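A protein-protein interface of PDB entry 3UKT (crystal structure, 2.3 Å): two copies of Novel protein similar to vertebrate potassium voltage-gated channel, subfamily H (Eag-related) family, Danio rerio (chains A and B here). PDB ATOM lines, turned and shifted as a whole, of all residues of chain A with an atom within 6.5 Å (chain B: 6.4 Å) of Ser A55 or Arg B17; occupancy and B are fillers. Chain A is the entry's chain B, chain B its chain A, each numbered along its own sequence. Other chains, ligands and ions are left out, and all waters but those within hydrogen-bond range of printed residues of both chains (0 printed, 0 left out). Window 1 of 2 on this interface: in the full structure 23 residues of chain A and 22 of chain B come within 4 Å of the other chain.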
ATOM      1  N   ILE A  52     -11.704 -38.681  15.680  1.00  0.00           N
ATOM      2  CA  ILE A  52     -13.001 -38.082  15.378  1.00  0.00           C
ATOM      3  C   ILE A  52     -12.902 -36.616  14.980  1.00  0.00           C
ATOM      4  O   ILE A  52     -11.956 -35.920  15.352  1.00  0.00           O
ATOM      5  CB  ILE A  52     -14.011 -38.197  16.532  1.00  0.00           C
ATOM      6  CG1 ILE A  52     -13.516 -37.443  17.766  1.00  0.00           C
ATOM      7  CG2 ILE A  52     -14.335 -39.643  16.838  1.00  0.00           C
ATOM      8  CD1 ILE A  52     -14.619 -37.276  18.820  1.00  0.00           C
ATOM      9  N   ASP A  53     -13.888 -36.170  14.207  1.00  0.00           N
ATOM     10  CA  ASP A  53     -14.010 -34.773  13.808  1.00  0.00           C
ATOM     11  C   ASP A  53     -14.690 -33.935  14.900  1.00  0.00           C
ATOM     12  O   ASP A  53     -15.874 -34.104  15.184  1.00  0.00           O
ATOM     13  CB  ASP A  53     -14.809 -34.714  12.513  1.00  0.00           C
ATOM     14  CG  ASP A  53     -15.138 -33.305  12.092  1.00  0.00           C
ATOM     15  OD1 ASP A  53     -14.494 -32.359  12.594  1.00  0.00           O
ATOM     16  OD2 ASP A  53     -16.047 -33.157  11.242  1.00  0.00           O
ATOM     17  N   VAL A  54     -13.946 -33.036  15.530  1.00  0.00           N
ATOM     18  CA  VAL A  54     -14.539 -32.215  16.586  1.00  0.00           C
ATOM     19  C   VAL A  54     -14.853 -30.804  16.098  1.00  0.00           C
ATOM     20  O   VAL A  54     -15.239 -29.946  16.876  1.00  0.00           O
ATOM     21  CB  VAL A  54     -13.651 -32.159  17.828  1.00  0.00           C
ATOM     22  CG1 VAL A  54     -13.475 -33.555  18.404  1.00  0.00           C
ATOM     23  CG2 VAL A  54     -12.291 -31.550  17.487  1.00  0.00           C
ATOM     24  N   SER A  55     -14.700 -30.570  14.801  1.00  0.00           N
ATOM     25  CA  SER A  55     -15.013 -29.258  14.247  1.00  0.00           C
ATOM     26  C   SER A  55     -16.505 -28.981  14.421  1.00  0.00           C
ATOM     27  O   SER A  55     -17.317 -29.901  14.442  1.00  0.00           O
ATOM     28  CB  SER A  55     -14.627 -29.180  12.766  1.00  0.00           C
ATOM     29  OG  SER A  55     -15.602 -29.795  11.943  1.00  0.00           O
ATOM     30  N   GLU A  56     -16.865 -27.720  14.570  1.00  0.00           N
ATOM     31  CA  GLU A  56     -18.268 -27.367  14.740  1.00  0.00           C
ATOM     32  C   GLU A  56     -18.522 -26.205  13.791  1.00  0.00           C
ATOM     33  O   GLU A  56     -18.400 -25.039  14.159  1.00  0.00           O
ATOM     34  CB  GLU A  56     -18.576 -27.022  16.209  1.00  0.00           C
ATOM     35  CG  GLU A  56     -20.079 -27.030  16.557  1.00  0.00           C
ATOM     36  CD  GLU A  56     -20.414 -26.627  18.019  1.00  0.00           C
ATOM     37  OE1 GLU A  56     -19.668 -27.017  18.954  1.00  0.00           O
ATOM     38  OE2 GLU A  56     -21.446 -25.930  18.227  1.00  0.00           O
ATOM     39  N   LEU A  57     -18.851 -26.556  12.554  1.00  0.00           N
ATOM     40  CA  LEU A  57     -18.889 -25.652  11.410  1.00  0.00           C
ATOM     41  C   LEU A  57     -19.994 -24.601  11.512  1.00  0.00           C
ATOM     42  O   LEU A  57     -19.830 -23.462  11.095  1.00  0.00           O
ATOM     43  CB  LEU A  57     -19.113 -26.491  10.149  1.00  0.00           C
ATOM     44  CG  LEU A  57     -18.330 -26.225   8.861  1.00  0.00           C
ATOM     45  CD1 LEU A  57     -16.843 -26.036   9.142  1.00  0.00           C
ATOM     46  CD2 LEU A  57     -18.557 -27.384   7.923  1.00  0.00           C
ATOM     47  N   ILE A  97     -24.573 -31.252  15.589  1.00  0.00           N
ATOM     48  CA  ILE A  97     -23.228 -31.717  15.931  1.00  0.00           C
ATOM     49  C   ILE A  97     -23.041 -33.245  15.782  1.00  0.00           C
ATOM     50  O   ILE A  97     -21.983 -33.773  16.072  1.00  0.00           O
ATOM     51  CB  ILE A  97     -22.808 -31.295  17.353  1.00  0.00           C
ATOM     52  CG1 ILE A  97     -23.743 -31.920  18.396  1.00  0.00           C
ATOM     53  CG2 ILE A  97     -22.755 -29.773  17.460  1.00  0.00           C
ATOM     54  CD1 ILE A  97     -23.295 -31.677  19.885  1.00  0.00           C
ATOM     55  N   LYS A  99     -21.923 -36.246  13.804  1.00  0.00           N
ATOM     56  CA  LYS A  99     -21.070 -36.574  12.669  1.00  0.00           C
ATOM     57  C   LYS A  99     -21.331 -38.009  12.191  1.00  0.00           C
ATOM     58  O   LYS A  99     -22.044 -38.791  12.852  1.00  0.00           O
ATOM     59  CB  LYS A  99     -19.603 -36.488  13.095  1.00  0.00           C
ATOM     60  CG  LYS A  99     -19.174 -35.196  13.749  1.00  0.00           C
ATOM     61  CD  LYS A  99     -19.193 -34.072  12.762  1.00  0.00           C
ATOM     62  CE  LYS A  99     -18.529 -32.845  13.360  1.00  0.00           C
ATOM     63  NZ  LYS A  99     -18.471 -31.803  12.282  1.00  0.00           N
ATOM     64  N   SER B  12      -5.020 -23.010   2.558  1.00  0.00           N
ATOM     65  CA  SER B  12      -5.848 -22.136   3.371  1.00  0.00           C
ATOM     66  C   SER B  12      -6.827 -22.945   4.211  1.00  0.00           C
ATOM     67  O   SER B  12      -7.516 -23.829   3.697  1.00  0.00           O
ATOM     68  CB  SER B  12      -6.623 -21.172   2.470  1.00  0.00           C
ATOM     69  OG  SER B  12      -7.567 -20.411   3.211  1.00  0.00           O
ATOM     70  N   LEU B  13      -6.879 -22.640   5.501  1.00  0.00           N
ATOM     71  CA  LEU B  13      -7.820 -23.270   6.402  1.00  0.00           C
ATOM     72  C   LEU B  13      -9.217 -22.865   5.970  1.00  0.00           C
ATOM     73  O   LEU B  13     -10.160 -23.658   6.013  1.00  0.00           O
ATOM     74  CB  LEU B  13      -7.577 -22.753   7.809  1.00  0.00           C
ATOM     75  CG  LEU B  13      -7.332 -23.704   8.979  1.00  0.00           C
ATOM     76  CD1 LEU B  13      -7.533 -22.915  10.275  1.00  0.00           C
ATOM     77  CD2 LEU B  13      -8.231 -24.922   8.930  1.00  0.00           C
ATOM     78  N   TYR B  14      -9.332 -21.605   5.567  1.00  0.00           N
ATOM     79  CA  TYR B  14     -10.577 -21.074   5.049  1.00  0.00           C
ATOM     80  C   TYR B  14     -11.103 -21.884   3.861  1.00  0.00           C
ATOM     81  O   TYR B  14     -12.301 -22.185   3.786  1.00  0.00           O
ATOM     82  CB  TYR B  14     -10.410 -19.612   4.631  1.00  0.00           C
ATOM     83  CG  TYR B  14     -11.650 -19.069   3.963  1.00  0.00           C
ATOM     84  CD1 TYR B  14     -12.780 -18.751   4.703  1.00  0.00           C
ATOM     85  CD2 TYR B  14     -11.701 -18.897   2.589  1.00  0.00           C
ATOM     86  CE1 TYR B  14     -13.919 -18.267   4.094  1.00  0.00           C
ATOM     87  CE2 TYR B  14     -12.828 -18.404   1.973  1.00  0.00           C
ATOM     88  CZ  TYR B  14     -13.936 -18.090   2.728  1.00  0.00           C
ATOM     89  OH  TYR B  14     -15.070 -17.607   2.103  1.00  0.00           O
ATOM     90  N   HIS B  15     -10.210 -22.226   2.931  1.00  0.00           N
ATOM     91  CA  HIS B  15     -10.593 -23.000   1.751  1.00  0.00           C
ATOM     92  C   HIS B  15     -10.965 -24.407   2.164  1.00  0.00           C
ATOM     93  O   HIS B  15     -11.940 -24.957   1.697  1.00  0.00           O
ATOM     94  CB  HIS B  15      -9.471 -23.035   0.708  1.00  0.00           C
ATOM     95  CG  HIS B  15      -9.229 -21.720   0.039  1.00  0.00           C
ATOM     96  ND1 HIS B  15     -10.126 -20.676   0.081  1.00  0.00           N
ATOM     97  CD2 HIS B  15      -8.171 -21.269  -0.697  1.00  0.00           C
ATOM     98  CE1 HIS B  15      -9.646 -19.642  -0.593  1.00  0.00           C
ATOM     99  NE2 HIS B  15      -8.459 -19.986  -1.074  1.00  0.00           N
ATOM    100  N   THR B  16     -10.173 -24.977   3.054  1.00  0.00           N
ATOM    101  CA  THR B  16     -10.472 -26.279   3.624  1.00  0.00           C
ATOM    102  C   THR B  16     -11.875 -26.320   4.233  1.00  0.00           C
ATOM    103  O   THR B  16     -12.728 -27.104   3.790  1.00  0.00           O
ATOM    104  CB  THR B  16      -9.414 -26.661   4.687  1.00  0.00           C
ATOM    105  OG1 THR B  16      -8.127 -26.719   4.060  1.00  0.00           O
ATOM    106  CG2 THR B  16      -9.736 -28.010   5.327  1.00  0.00           C
ATOM    107  N   ARG B  17     -12.120 -25.463   5.221  1.00  0.00           N
ATOM    108  CA  ARG B  17     -13.435 -25.391   5.879  1.00  0.00           C
ATOM    109  C   ARG B  17     -14.574 -25.128   4.912  1.00  0.00           C
ATOM    110  O   ARG B  17     -15.670 -25.636   5.087  1.00  0.00           O
ATOM    111  CB  ARG B  17     -13.450 -24.328   6.967  1.00  0.00           C
ATOM    112  CG  ARG B  17     -12.365 -24.506   8.024  1.00  0.00           C
ATOM    113  CD  ARG B  17     -12.562 -25.785   8.791  1.00  0.00           C
ATOM    114  NE  ARG B  17     -11.763 -25.849  10.015  1.00  0.00           N
ATOM    115  CZ  ARG B  17     -11.585 -26.970  10.717  1.00  0.00           C
ATOM    116  NH1 ARG B  17     -12.146 -28.104  10.294  1.00  0.00           N
ATOM    117  NH2 ARG B  17     -10.849 -26.970  11.829  1.00  0.00           N
ATOM    118  N   THR B  18     -14.313 -24.335   3.890  1.00  0.00           N
ATOM    119  CA  THR B  18     -15.326 -24.067   2.880  1.00  0.00           C
ATOM    120  C   THR B  18     -15.717 -25.367   2.180  1.00  0.00           C
ATOM    121  O   THR B  18     -16.905 -25.637   1.992  1.00  0.00           O
ATOM    122  CB  THR B  18     -14.823 -23.030   1.863  1.00  0.00           C
ATOM    123  OG1 THR B  18     -14.870 -21.742   2.476  1.00  0.00           O
ATOM    124  CG2 THR B  18     -15.684 -23.009   0.617  1.00  0.00           C
ATOM    125  N   LYS B  19     -14.715 -26.177   1.833  1.00  0.00           N
ATOM    126  CA  LYS B  19     -14.951 -27.455   1.186  1.00  0.00           C
ATOM    127  C   LYS B  19     -15.737 -28.368   2.126  1.00  0.00           C
ATOM    128  O   LYS B  19     -16.670 -29.035   1.697  1.00  0.00           O
ATOM    129  CB  LYS B  19     -13.635 -28.103   0.750  1.00  0.00           C
ATOM    130  N   ASP B  20     -15.398 -28.359   3.413  1.00  0.00           N
ATOM    131  CA  ASP B  20     -16.121 -29.174   4.372  1.00  0.00           C
ATOM    132  C   ASP B  20     -17.584 -28.768   4.472  1.00  0.00           C
ATOM    133  O   ASP B  20     -18.465 -29.625   4.641  1.00  0.00           O
ATOM    134  CB  ASP B  20     -15.484 -29.091   5.759  1.00  0.00           C
ATOM    135  CG  ASP B  20     -14.071 -29.642   5.786  1.00  0.00           C
ATOM    136  OD1 ASP B  20     -13.701 -30.415   4.861  1.00  0.00           O
ATOM    137  OD2 ASP B  20     -13.322 -29.303   6.732  1.00  0.00           O
ATOM    138  N   LEU B  21     -17.844 -27.465   4.388  1.00  0.00           N
ATOM    139  CA  LEU B  21     -19.215 -26.958   4.412  1.00  0.00           C
ATOM    140  C   LEU B  21     -19.917 -27.395   3.131  1.00  0.00           C
ATOM    141  O   LEU B  21     -21.079 -27.749   3.151  1.00  0.00           O
ATOM    142  CB  LEU B  21     -19.246 -25.419   4.539  1.00  0.00           C
ATOM    143  CG  LEU B  21     -20.634 -24.767   4.706  1.00  0.00           C
ATOM    144  CD1 LEU B  21     -21.420 -25.398   5.871  1.00  0.00           C
ATOM    145  CD2 LEU B  21     -20.558 -23.259   4.890  1.00  0.00           C
ATOM    146  N   LYS B  22     -19.214 -27.378   2.009  1.00  0.00           N
ATOM    147  CA  LYS B  22     -19.858 -27.809   0.782  1.00  0.00           C
ATOM    148  C   LYS B  22     -20.172 -29.307   0.787  1.00  0.00           C
ATOM    149  O   LYS B  22     -21.250 -29.698   0.328  1.00  0.00           O
ATOM    150  CB  LYS B  22     -19.069 -27.387  -0.451  1.00  0.00           C
ATOM    151  CG  LYS B  22     -19.314 -25.918  -0.833  1.00  0.00           C
ATOM    152  CD  LYS B  22     -18.145 -25.325  -1.607  1.00  0.00           C
ATOM    153  CE  LYS B  22     -18.471 -23.944  -2.173  1.00  0.00           C
ATOM    154  NZ  LYS B  22     -17.284 -23.334  -2.825  1.00  0.00           N
ATOM    155  N   PHE B  42     -21.135 -18.063   5.841  1.00  0.00           N
ATOM    156  CA  PHE B  42     -19.859 -18.625   6.220  1.00  0.00           C
ATOM    157  C   PHE B  42     -18.742 -17.629   5.946  1.00  0.00           C
ATOM    158  O   PHE B  42     -17.890 -17.406   6.797  1.00  0.00           O
ATOM    159  CB  PHE B  42     -19.587 -19.943   5.516  1.00  0.00           C
ATOM    160  CG  PHE B  42     -18.273 -20.575   5.905  1.00  0.00           C
ATOM    161  CD1 PHE B  42     -18.130 -21.230   7.130  1.00  0.00           C
ATOM    162  CD2 PHE B  42     -17.189 -20.518   5.049  1.00  0.00           C
ATOM    163  CE1 PHE B  42     -16.933 -21.800   7.485  1.00  0.00           C
ATOM    164  CE2 PHE B  42     -15.989 -21.106   5.406  1.00  0.00           C
ATOM    165  CZ  PHE B  42     -15.864 -21.745   6.619  1.00  0.00           C
ATOM    166  N   TRP B  46     -16.678 -15.771   9.080  1.00  0.00           N
ATOM    167  CA  TRP B  46     -15.476 -16.596   9.171  1.00  0.00           C
ATOM    168  C   TRP B  46     -14.336 -15.894   9.875  1.00  0.00           C
ATOM    169  O   TRP B  46     -14.112 -14.712   9.669  1.00  0.00           O
ATOM    170  CB  TRP B  46     -14.983 -17.008   7.779  1.00  0.00           C
ATOM    171  CG  TRP B  46     -13.555 -17.452   7.775  1.00  0.00           C
ATOM    172  CD1 TRP B  46     -12.469 -16.719   7.397  1.00  0.00           C
ATOM    173  CD2 TRP B  46     -13.053 -18.732   8.180  1.00  0.00           C
ATOM    174  NE1 TRP B  46     -11.320 -17.464   7.528  1.00  0.00           N
ATOM    175  CE2 TRP B  46     -11.648 -18.703   8.010  1.00  0.00           C
ATOM    176  CE3 TRP B  46     -13.655 -19.909   8.645  1.00  0.00           C
ATOM    177  CZ2 TRP B  46     -10.832 -19.796   8.304  1.00  0.00           C
ATOM    178  CZ3 TRP B  46     -12.843 -20.999   8.935  1.00  0.00           C
ATOM    179  CH2 TRP B  46     -11.442 -20.934   8.763  1.00  0.00           C
ATOM    180  N   GLY B  51     -11.995 -21.275  13.479  1.00  0.00           N
ATOM    181  CA  GLY B  51     -11.952 -22.497  12.701  1.00  0.00           C
ATOM    182  C   GLY B  51     -10.613 -23.214  12.702  1.00  0.00           C
ATOM    183  O   GLY B  51     -10.324 -23.948  11.765  1.00  0.00           O
ATOM    184  N   ILE B  52      -9.796 -23.027  13.738  1.00  0.00           N
ATOM    185  CA  ILE B  52      -8.445 -23.594  13.731  1.00  0.00           C
ATOM    186  C   ILE B  52      -8.444 -25.121  13.750  1.00  0.00           C
ATOM    187  O   ILE B  52      -9.421 -25.757  14.154  1.00  0.00           O
ATOM    188  CB  ILE B  52      -7.570 -23.125  14.920  1.00  0.00           C
ATOM    189  CG1 ILE B  52      -8.181 -23.568  16.247  1.00  0.00           C
ATOM    190  CG2 ILE B  52      -7.305 -21.625  14.874  1.00  0.00           C
ATOM    191  CD1 ILE B  52      -7.203 -23.532  17.411  1.00  0.00           C
ATOM    192  N   ASP B  53      -7.330 -25.702  13.329  1.00  0.00           N
ATOM    193  CA  ASP B  53      -7.191 -27.150  13.329  1.00  0.00           C
ATOM    194  C   ASP B  53      -6.639 -27.682  14.660  1.00  0.00           C
ATOM    195  O   ASP B  53      -5.495 -27.426  15.010  1.00  0.00           O
ATOM    196  CB  ASP B  53      -6.292 -27.580  12.179  1.00  0.00           C
ATOM    197  CG  ASP B  53      -6.115 -29.070  12.124  1.00  0.00           C
ATOM    198  OD1 ASP B  53      -6.920 -29.779  12.767  1.00  0.00           O
ATOM    199  OD2 ASP B  53      -5.176 -29.525  11.440  1.00  0.00           O
ATOM    200  N   VAL B  54      -7.463 -28.426  15.390  1.00  0.00           N
ATOM    201  CA  VAL B  54      -7.070 -28.996  16.667  1.00  0.00           C
ATOM    202  C   VAL B  54      -6.696 -30.488  16.550  1.00  0.00           C
ATOM    203  O   VAL B  54      -6.411 -31.154  17.558  1.00  0.00           O
ATOM    204  CB  VAL B  54      -8.211 -28.839  17.704  1.00  0.00           C
ATOM    205  CG1 VAL B  54      -8.665 -27.384  17.783  1.00  0.00           C
ATOM    206  CG2 VAL B  54      -9.406 -29.749  17.354  1.00  0.00           C
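Among the printed residues, pairs that only touch across the chains: Val A54 with Val B54 (3.4 Å), Leu A57 with Leu B21 (3.6 Å), Ser A55 with Arg B17 (3.7 Å) and Leu A57 with Asp B20 (3.8 Å).
Printed residues of chain B within 4 Å of Val A54: Val B54.
Ser A55 touches one residue of chain B.
Of the printed residues of chain B, Leu A57 touches Asp B20 (3.8 Å) and Leu B21 (3.6 Å).
Thr B16 touches none of the printed residues of chain A.
Arg B17 touches just one residue of chain A: Ser A55 (3.7 Å).
Printed residues of chain A within 4 Å of Leu B21: Leu A57 (3.6 Å).
Printed residues of chain A within 4 Å of Val B54: Val A54 (3.4 Å).
The nearest residue of chain B that does not touch Ser A55 is Asp B20 (5.7 Å).
The nearest residue of chain A that does not touch Arg B17 is Leu A57 (4.2 Å).
Printed residues of chain B that touch a printed residue of chain A: Arg B17, Asp B20, Leu B21 and Val B54.
Hydrophobic or aromatic side chains of chain B that line the printed part of chain A: Leu B21 and Val B54.
Along chain B the printed residues that touch a printed residue of chain A span positions 17 to 54.
Of the 8 printed residues of chain A, 3 touch a printed residue of chain B.
Among the printed residues, 4 pairs touch across the chains.
Among the printed residues, no Asp or Glu carboxylate lies within 4 Å of a Lys or Arg side-chain nitrogen of the other chain.
NH2 of Arg B17 is in hydrogen-bond range of O of Ile B52, 3.0 Å away.
NE of Arg B17 lies within hydrogen-bond range of O of Gly B51 (3.0 Å).
The backbone NH (N) of Ser A55 is in hydrogen-bond range of the side-chain carboxylate (OD1) of Asp A53, at 2.8 Å.
NH1 of Arg B17 is in salt-bridge range of OD2 of Asp B20, 3.9 Å away.
The side-chain amino group (NZ) of Lys A99 lies within hydrogen-bond range of the backbone carbonyl oxygen (O) of Ser A55, at 3.1 Å.
Val A54 touches its own counterpart, Val B54.
Of the 4 pairs that touch across the chains among the printed residues, 1 has its exchanged pair printed and touching as well.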
